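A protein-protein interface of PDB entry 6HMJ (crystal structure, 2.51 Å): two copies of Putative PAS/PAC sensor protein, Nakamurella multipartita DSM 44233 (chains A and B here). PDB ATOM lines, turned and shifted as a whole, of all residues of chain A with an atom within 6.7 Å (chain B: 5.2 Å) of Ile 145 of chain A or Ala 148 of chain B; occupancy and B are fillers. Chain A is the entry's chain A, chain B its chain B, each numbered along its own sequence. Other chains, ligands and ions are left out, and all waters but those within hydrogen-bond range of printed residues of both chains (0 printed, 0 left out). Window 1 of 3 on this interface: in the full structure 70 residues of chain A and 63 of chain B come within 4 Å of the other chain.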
ATOM      1  N   ASP A 140     -13.971   8.832  21.759  1.00  0.00           N
ATOM      2  CA  ASP A 140     -14.389  10.229  21.774  1.00  0.00           C
ATOM      3  C   ASP A 140     -13.187  11.166  21.756  1.00  0.00           C
ATOM      4  O   ASP A 140     -13.207  12.198  21.075  1.00  0.00           O
ATOM      5  CB  ASP A 140     -15.266  10.501  22.997  1.00  0.00           C
ATOM      6  CG  ASP A 140     -16.650   9.894  22.866  1.00  0.00           C
ATOM      7  OD1 ASP A 140     -17.067   9.608  21.723  1.00  0.00           O
ATOM      8  OD2 ASP A 140     -17.323   9.706  23.902  1.00  0.00           O
ATOM      9  N   GLN A 141     -12.134  10.831  22.506  1.00  0.00           N
ATOM     10  CA  GLN A 141     -10.928  11.653  22.499  1.00  0.00           C
ATOM     11  C   GLN A 141     -10.266  11.630  21.126  1.00  0.00           C
ATOM     12  O   GLN A 141      -9.891  12.678  20.585  1.00  0.00           O
ATOM     13  CB  GLN A 141      -9.954  11.171  23.573  1.00  0.00           C
ATOM     14  CG  GLN A 141      -8.684  12.004  23.674  1.00  0.00           C
ATOM     15  CD  GLN A 141      -7.796  11.574  24.823  1.00  0.00           C
ATOM     16  OE1 GLN A 141      -8.183  10.745  25.643  1.00  0.00           O
ATOM     17  NE2 GLN A 141      -6.594  12.132  24.883  1.00  0.00           N
ATOM     18  N   ALA A 142     -10.111  10.438  20.546  1.00  0.00           N
ATOM     19  CA  ALA A 142      -9.517  10.334  19.218  1.00  0.00           C
ATOM     20  C   ALA A 142     -10.383  11.036  18.180  1.00  0.00           C
ATOM     21  O   ALA A 142      -9.863  11.676  17.259  1.00  0.00           O
ATOM     22  CB  ALA A 142      -9.307   8.866  18.844  1.00  0.00           C
ATOM     23  N   LYS A 143     -11.710  10.922  18.306  1.00  0.00           N
ATOM     24  CA  LYS A 143     -12.590  11.633  17.387  1.00  0.00           C
ATOM     25  C   LYS A 143     -12.318  13.132  17.442  1.00  0.00           C
ATOM     26  O   LYS A 143     -12.242  13.798  16.403  1.00  0.00           O
ATOM     27  CB  LYS A 143     -14.058  11.372  17.733  1.00  0.00           C
ATOM     28  CG  LYS A 143     -15.031  11.929  16.698  1.00  0.00           C
ATOM     29  CD  LYS A 143     -16.483  11.941  17.172  1.00  0.00           C
ATOM     30  CE  LYS A 143     -17.018  10.585  17.581  1.00  0.00           C
ATOM     31  NZ  LYS A 143     -18.457  10.707  17.967  1.00  0.00           N
ATOM     32  N   GLY A 144     -12.152  13.675  18.650  1.00  0.00           N
ATOM     33  CA  GLY A 144     -11.883  15.096  18.785  1.00  0.00           C
ATOM     34  C   GLY A 144     -10.514  15.489  18.268  1.00  0.00           C
ATOM     35  O   GLY A 144     -10.354  16.547  17.653  1.00  0.00           O
ATOM     36  N   ILE A 145      -9.506  14.650  18.517  1.00  0.00           N
ATOM     37  CA  ILE A 145      -8.165  14.925  18.009  1.00  0.00           C
ATOM     38  C   ILE A 145      -8.193  15.046  16.490  1.00  0.00           C
ATOM     39  O   ILE A 145      -7.613  15.972  15.911  1.00  0.00           O
ATOM     40  CB  ILE A 145      -7.184  13.832  18.470  1.00  0.00           C
ATOM     41  CG1 ILE A 145      -6.918  13.962  19.970  1.00  0.00           C
ATOM     42  CG2 ILE A 145      -5.883  13.922  17.689  1.00  0.00           C
ATOM     43  CD1 ILE A 145      -6.105  12.824  20.557  1.00  0.00           C
ATOM     44  N   VAL A 146      -8.864  14.106  15.823  1.00  0.00           N
ATOM     45  CA  VAL A 146      -8.954  14.148  14.368  1.00  0.00           C
ATOM     46  C   VAL A 146      -9.744  15.370  13.913  1.00  0.00           C
ATOM     47  O   VAL A 146      -9.389  16.020  12.922  1.00  0.00           O
ATOM     48  CB  VAL A 146      -9.574  12.841  13.838  1.00  0.00           C
ATOM     49  CG1 VAL A 146      -9.959  12.986  12.374  1.00  0.00           C
ATOM     50  CG2 VAL A 146      -8.603  11.681  14.027  1.00  0.00           C
ATOM     51  N   MET A 147     -10.831  15.694  14.618  1.00  0.00           N
ATOM     52  CA  MET A 147     -11.652  16.843  14.249  1.00  0.00           C
ATOM     53  C   MET A 147     -10.812  18.109  14.130  1.00  0.00           C
ATOM     54  O   MET A 147     -10.857  18.809  13.112  1.00  0.00           O
ATOM     55  CB  MET A 147     -12.762  17.046  15.282  1.00  0.00           C
ATOM     56  CG  MET A 147     -13.954  16.116  15.125  1.00  0.00           C
ATOM     57  SD  MET A 147     -15.217  16.421  16.374  1.00  0.00           S
ATOM     58  CE  MET A 147     -15.766  18.059  15.908  1.00  0.00           C
ATOM     59  N   ALA A 148     -10.041  18.425  15.172  1.00  0.00           N
ATOM     60  CA  ALA A 148      -9.307  19.683  15.199  1.00  0.00           C
ATOM     61  C   ALA A 148      -7.979  19.597  14.455  1.00  0.00           C
ATOM     62  O   ALA A 148      -7.557  20.583  13.842  1.00  0.00           O
ATOM     63  CB  ALA A 148      -9.078  20.115  16.649  1.00  0.00           C
ATOM     64  N   ALA A 149      -7.311  18.441  14.493  1.00  0.00           N
ATOM     65  CA  ALA A 149      -6.025  18.304  13.814  1.00  0.00           C
ATOM     66  C   ALA A 149      -6.163  18.573  12.321  1.00  0.00           C
ATOM     67  O   ALA A 149      -5.353  19.299  11.731  1.00  0.00           O
ATOM     68  CB  ALA A 149      -5.446  16.911  14.057  1.00  0.00           C
ATOM     69  N   PHE A 150      -7.179  17.986  11.689  1.00  0.00           N
ATOM     70  CA  PHE A 150      -7.438  18.180  10.270  1.00  0.00           C
ATOM     71  C   PHE A 150      -8.582  19.150  10.002  1.00  0.00           C
ATOM     72  O   PHE A 150      -8.963  19.330   8.841  1.00  0.00           O
ATOM     73  CB  PHE A 150      -7.755  16.839   9.593  1.00  0.00           C
ATOM     74  CG  PHE A 150      -6.647  15.826   9.683  1.00  0.00           C
ATOM     75  CD1 PHE A 150      -5.521  15.944   8.888  1.00  0.00           C
ATOM     76  CD2 PHE A 150      -6.743  14.745  10.543  1.00  0.00           C
ATOM     77  CE1 PHE A 150      -4.506  15.012   8.961  1.00  0.00           C
ATOM     78  CE2 PHE A 150      -5.726  13.807  10.615  1.00  0.00           C
ATOM     79  CZ  PHE A 150      -4.611  13.942   9.826  1.00  0.00           C
ATOM     80  N   ASP A 151      -9.137  19.771  11.039  1.00  0.00           N
ATOM     81  CA  ASP A 151     -10.248  20.711  10.903  1.00  0.00           C
ATOM     82  C   ASP A 151     -11.376  20.112  10.061  1.00  0.00           C
ATOM     83  O   ASP A 151     -11.724  20.605   8.986  1.00  0.00           O
ATOM     84  CB  ASP A 151      -9.766  22.037  10.311  1.00  0.00           C
ATOM     85  CG  ASP A 151     -10.847  23.106  10.311  1.00  0.00           C
ATOM     86  OD1 ASP A 151     -11.432  23.361  11.383  1.00  0.00           O
ATOM     87  OD2 ASP A 151     -11.107  23.695   9.238  1.00  0.00           O
ATOM     88  N   ALA A 157     -14.559  13.117  10.988  1.00  0.00           N
ATOM     89  CA  ALA A 157     -13.519  12.590  11.864  1.00  0.00           C
ATOM     90  C   ALA A 157     -13.791  11.132  12.208  1.00  0.00           C
ATOM     91  O   ALA A 157     -12.887  10.289  12.162  1.00  0.00           O
ATOM     92  CB  ALA A 157     -13.430  13.431  13.136  1.00  0.00           C
ATOM     93  N   MET A 179      -3.725   5.487  18.160  1.00  0.00           N
ATOM     94  CA  MET A 179      -3.509   6.850  17.688  1.00  0.00           C
ATOM     95  C   MET A 179      -3.163   7.784  18.841  1.00  0.00           C
ATOM     96  O   MET A 179      -2.313   8.671  18.695  1.00  0.00           O
ATOM     97  CB  MET A 179      -4.753   7.355  16.956  1.00  0.00           C
ATOM     98  CG  MET A 179      -4.561   8.691  16.264  1.00  0.00           C
ATOM     99  SD  MET A 179      -6.125   9.493  15.868  1.00  0.00           S
ATOM    100  CE  MET A 179      -6.445  10.330  17.419  1.00  0.00           C
ATOM    101  N   ILE A 180      -3.811   7.604  19.992  1.00  0.00           N
ATOM    102  CA  ILE A 180      -3.557   8.479  21.131  1.00  0.00           C
ATOM    103  C   ILE A 180      -2.175   8.205  21.712  1.00  0.00           C
ATOM    104  O   ILE A 180      -1.370   9.123  21.903  1.00  0.00           O
ATOM    105  CB  ILE A 180      -4.663   8.309  22.189  1.00  0.00           C
ATOM    106  CG1 ILE A 180      -6.024   8.674  21.587  1.00  0.00           C
ATOM    107  CG2 ILE A 180      -4.367   9.165  23.412  1.00  0.00           C
ATOM    108  CD1 ILE A 180      -7.208   8.354  22.481  1.00  0.00           C
ATOM    109  N   LEU A 183       0.502   9.267  19.019  1.00  0.00           N
ATOM    110  CA  LEU A 183       0.624  10.716  18.899  1.00  0.00           C
ATOM    111  C   LEU A 183       1.348  11.303  20.103  1.00  0.00           C
ATOM    112  O   LEU A 183       2.180  12.208  19.957  1.00  0.00           O
ATOM    113  CB  LEU A 183      -0.763  11.343  18.745  1.00  0.00           C
ATOM    114  CG  LEU A 183      -0.840  12.870  18.723  1.00  0.00           C
ATOM    115  CD1 LEU A 183      -0.091  13.437  17.531  1.00  0.00           C
ATOM    116  CD2 LEU A 183      -2.287  13.322  18.707  1.00  0.00           C
ATOM    117  N   LEU A 192       1.571  19.207  13.242  1.00  0.00           N
ATOM    118  CA  LEU A 192       0.640  18.223  13.789  1.00  0.00           C
ATOM    119  C   LEU A 192       0.120  17.260  12.725  1.00  0.00           C
ATOM    120  O   LEU A 192       0.104  16.041  12.937  1.00  0.00           O
ATOM    121  CB  LEU A 192      -0.525  18.940  14.476  1.00  0.00           C
ATOM    122  CG  LEU A 192      -1.616  18.038  15.058  1.00  0.00           C
ATOM    123  CD1 LEU A 192      -1.020  17.007  16.003  1.00  0.00           C
ATOM    124  CD2 LEU A 192      -2.669  18.872  15.775  1.00  0.00           C
ATOM    125  N   LEU A 196       0.529  13.343  12.858  1.00  0.00           N
ATOM    126  CA  LEU A 196      -0.554  12.378  13.012  1.00  0.00           C
ATOM    127  C   LEU A 196      -0.590  11.395  11.848  1.00  0.00           C
ATOM    128  O   LEU A 196      -0.877  10.208  12.040  1.00  0.00           O
ATOM    129  CB  LEU A 196      -1.884  13.119  13.139  1.00  0.00           C
ATOM    130  CG  LEU A 196      -3.115  12.322  13.570  1.00  0.00           C
ATOM    131  CD1 LEU A 196      -2.870  11.562  14.862  1.00  0.00           C
ATOM    132  CD2 LEU A 196      -4.293  13.271  13.720  1.00  0.00           C
ATOM    133  N   LYS B 143     -11.776  17.340  25.190  1.00  0.00           N
ATOM    134  CA  LYS B 143     -10.352  17.243  25.490  1.00  0.00           C
ATOM    135  C   LYS B 143      -9.548  17.031  24.214  1.00  0.00           C
ATOM    136  O   LYS B 143      -8.525  17.685  23.991  1.00  0.00           O
ATOM    137  CB  LYS B 143     -10.083  16.082  26.450  1.00  0.00           C
ATOM    138  CG  LYS B 143      -8.649  16.060  26.966  1.00  0.00           C
ATOM    139  CD  LYS B 143      -8.204  14.670  27.413  1.00  0.00           C
ATOM    140  CE  LYS B 143      -8.656  14.276  28.798  1.00  0.00           C
ATOM    141  NZ  LYS B 143      -8.007  12.982  29.173  1.00  0.00           N
ATOM    142  N   GLY B 144     -10.012  16.117  23.357  1.00  0.00           N
ATOM    143  CA  GLY B 144      -9.301  15.844  22.118  1.00  0.00           C
ATOM    144  C   GLY B 144      -9.274  17.031  21.176  1.00  0.00           C
ATOM    145  O   GLY B 144      -8.285  17.258  20.475  1.00  0.00           O
ATOM    146  N   ILE B 145     -10.362  17.798  21.138  1.00  0.00           N
ATOM    147  CA  ILE B 145     -10.411  18.964  20.265  1.00  0.00           C
ATOM    148  C   ILE B 145      -9.420  20.027  20.725  1.00  0.00           C
ATOM    149  O   ILE B 145      -8.704  20.618  19.909  1.00  0.00           O
ATOM    150  CB  ILE B 145     -11.848  19.516  20.200  1.00  0.00           C
ATOM    151  CG1 ILE B 145     -12.719  18.591  19.344  1.00  0.00           C
ATOM    152  CG2 ILE B 145     -11.855  20.937  19.658  1.00  0.00           C
ATOM    153  CD1 ILE B 145     -14.198  18.938  19.362  1.00  0.00           C
ATOM    154  N   VAL B 146      -9.355  20.284  22.033  1.00  0.00           N
ATOM    155  CA  VAL B 146      -8.474  21.334  22.536  1.00  0.00           C
ATOM    156  C   VAL B 146      -7.010  20.954  22.358  1.00  0.00           C
ATOM    157  O   VAL B 146      -6.188  21.780  21.942  1.00  0.00           O
ATOM    158  CB  VAL B 146      -8.799  21.636  24.011  1.00  0.00           C
ATOM    159  CG1 VAL B 146      -7.691  22.460  24.647  1.00  0.00           C
ATOM    160  CG2 VAL B 146     -10.121  22.368  24.117  1.00  0.00           C
ATOM    161  N   MET B 147      -6.651  19.708  22.676  1.00  0.00           N
ATOM    162  CA  MET B 147      -5.258  19.291  22.538  1.00  0.00           C
ATOM    163  C   MET B 147      -4.797  19.402  21.088  1.00  0.00           C
ATOM    164  O   MET B 147      -3.688  19.878  20.819  1.00  0.00           O
ATOM    165  CB  MET B 147      -5.067  17.884  23.109  1.00  0.00           C
ATOM    166  CG  MET B 147      -5.937  16.801  22.523  1.00  0.00           C
ATOM    167  SD  MET B 147      -5.795  15.247  23.452  1.00  0.00           S
ATOM    168  CE  MET B 147      -4.024  14.976  23.483  1.00  0.00           C
ATOM    169  N   ALA B 148      -5.637  18.986  20.139  1.00  0.00           N
ATOM    170  CA  ALA B 148      -5.249  19.042  18.733  1.00  0.00           C
ATOM    171  C   ALA B 148      -5.298  20.467  18.190  1.00  0.00           C
ATOM    172  O   ALA B 148      -4.476  20.835  17.343  1.00  0.00           O
ATOM    173  CB  ALA B 148      -6.157  18.131  17.902  1.00  0.00           C
ATOM    174  N   ALA B 149      -6.250  21.276  18.655  1.00  0.00           N
ATOM    175  CA  ALA B 149      -6.432  22.610  18.093  1.00  0.00           C
ATOM    176  C   ALA B 149      -5.254  23.521  18.420  1.00  0.00           C
ATOM    177  O   ALA B 149      -4.855  24.347  17.590  1.00  0.00           O
ATOM    178  CB  ALA B 149      -7.735  23.224  18.605  1.00  0.00           C
ATOM    179  N   PHE B 150      -4.692  23.396  19.622  1.00  0.00           N
ATOM    180  CA  PHE B 150      -3.553  24.201  20.044  1.00  0.00           C
ATOM    181  C   PHE B 150      -2.258  23.402  20.119  1.00  0.00           C
ATOM    182  O   PHE B 150      -1.256  23.914  20.625  1.00  0.00           O
ATOM    183  CB  PHE B 150      -3.843  24.845  21.402  1.00  0.00           C
ATOM    184  CG  PHE B 150      -5.091  25.678  21.422  1.00  0.00           C
ATOM    185  CD1 PHE B 150      -5.145  26.881  20.742  1.00  0.00           C
ATOM    186  CD2 PHE B 150      -6.211  25.256  22.118  1.00  0.00           C
ATOM    187  CE1 PHE B 150      -6.294  27.652  20.759  1.00  0.00           C
ATOM    188  CE2 PHE B 150      -7.361  26.021  22.136  1.00  0.00           C
ATOM    189  CZ  PHE B 150      -7.403  27.221  21.456  1.00  0.00           C
ATOM    190  N   ASP B 151      -2.255  22.165  19.632  1.00  0.00           N
ATOM    191  CA  ASP B 151      -1.079  21.301  19.680  1.00  0.00           C
ATOM    192  C   ASP B 151      -0.474  21.299  21.085  1.00  0.00           C
ATOM    193  O   ASP B 151       0.701  21.604  21.296  1.00  0.00           O
ATOM    194  CB  ASP B 151      -0.045  21.725  18.632  1.00  0.00           C
ATOM    195  CG  ASP B 151       1.048  20.687  18.434  1.00  0.00           C
ATOM    196  OD1 ASP B 151       0.926  19.577  18.993  1.00  0.00           O
ATOM    197  OD2 ASP B 151       2.030  20.982  17.718  1.00  0.00           O
ATOM    198  N   VAL B 152      -1.320  20.953  22.055  1.00  0.00           N
ATOM    199  CA  VAL B 152      -0.918  20.800  23.446  1.00  0.00           C
ATOM    200  C   VAL B 152      -1.276  19.382  23.879  1.00  0.00           C
ATOM    201  O   VAL B 152      -1.994  18.663  23.185  1.00  0.00           O
ATOM    202  CB  VAL B 152      -1.576  21.846  24.367  1.00  0.00           C
ATOM    203  CG1 VAL B 152      -1.008  23.233  24.080  1.00  0.00           C
ATOM    204  CG2 VAL B 152      -3.091  21.835  24.208  1.00  0.00           C
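The backbone carbonyl oxygen of Met 147 of chain B sits at hydrogen-bond distance from the backbone NH of Val 152 of chain B (2.9 Å).
The side-chain amide nitrogen (NE2) of Gln 141 of chain A sits at hydrogen-bond distance from the side-chain sulfur (SD) of Met 147 of chain B, at 3.5 Å.
The backbone carbonyl oxygen (O) of Gly 144 of chain B sits close to the backbone NH (N) of Ile 145 of chain A (3.5 Å).
Of the printed residues of chain B, Gln 141 of chain A touches Lys 143, Gly 144 and Met 147.
Of the printed residues of chain B, Gly 144 of chain A touches Gly 144 and Ile 145.
Printed residues of chain B within 4 Å of Ile 145 of chain A: Gly 144, Met 147 and Ala 148.
Asp 151 of chain A touches none of the printed residues of chain B.
Ile 180 of chain A touches none of the printed residues of chain B.
Printed residues of chain A within 4 Å of Ile 145 of chain B: Gly 144, Met 147 and Ala 148.
Printed residues of chain A within 4 Å of Met 147 of chain B: Gln 141 (3.5 Å) and Ile 145 (3.8 Å).
Ala 148 of chain B touches just these residues of chain A: Ile 145 (3.3 Å), Ala 148 (3.7 Å), Ala 149 (3.6 Å) and Leu 192 (3.1 Å).
The nearest residue of chain B that does not touch Ile 145 of chain A is Ile 145 of chain B (4.2 Å).
The nearest residue of chain A that does not touch Ala 148 of chain B is Gly 144 of chain A (4.5 Å).
The nearest printed residue of chain A that does not touch Ile 145 of chain B is Ile 145 of chain A (4.2 Å).
CD of Lys 143 of chain B touches NE2 of Gln 141 of chain A, 3.9 Å away.
Gln 141 of chain A touches Gly 144 of chain B (O to CA, 3.6 Å).
Gly 144 of chain B touches Gly 144 of chain A.
Ile 145 of chain B touches Gly 144 of chain A.
Ala 148 of chain B touches Ile 145 of chain A (CB to O, 3.3 Å).
Met 147 of chain A touches Ile 145 of chain B.
Ile 145 of chain B touches Ala 148 of chain A (O to CB, 3.3 Å).
Ala 148 of chain A touches Ala 148 of chain B.
Ala 149 of chain B touches Ala 148 of chain A.
Ala 148 of chain B touches Ala 149 of chain A.
Gly 144 of chain B touches its own counterpart, Gly 144 of chain A.
Ile 145 of chain A touches Met 147 of chain B, and with the chains exchanged Met 147 of chain A touches Ile 145 of chain B.
Ile 145 of chain A touches Ala 148 of chain B, and with the chains exchanged Ala 148 of chain A touches Ile 145 of chain B.
Ala 148 of chain A touches its own counterpart, Ala 148 of chain B.
Positions printed for both chains: 143, 144, 145, 146, 147, 148, 149, 150 and 151.
Of the 14 pairs that touch across the chains among the printed residues, 10 have their exchanged pair printed and touching as well.
Printed residues of chain A that touch a printed residue of chain B: Gln 141, Gly 144, Ile 145, Met 147, Ala 148, Ala 149 and Leu 192.
Hydrophobic or aromatic side chains of chain A that line the printed part of chain B: Ile 145, Met 147, Ala 148 and Leu 192.
Of the 10 printed residues of chain B, 6 touch a printed residue of chain A.
Hydrophobic or aromatic side chains of chain B that line the printed part of chain A: Ile 145, Met 147, Ala 148 and Ala 149.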
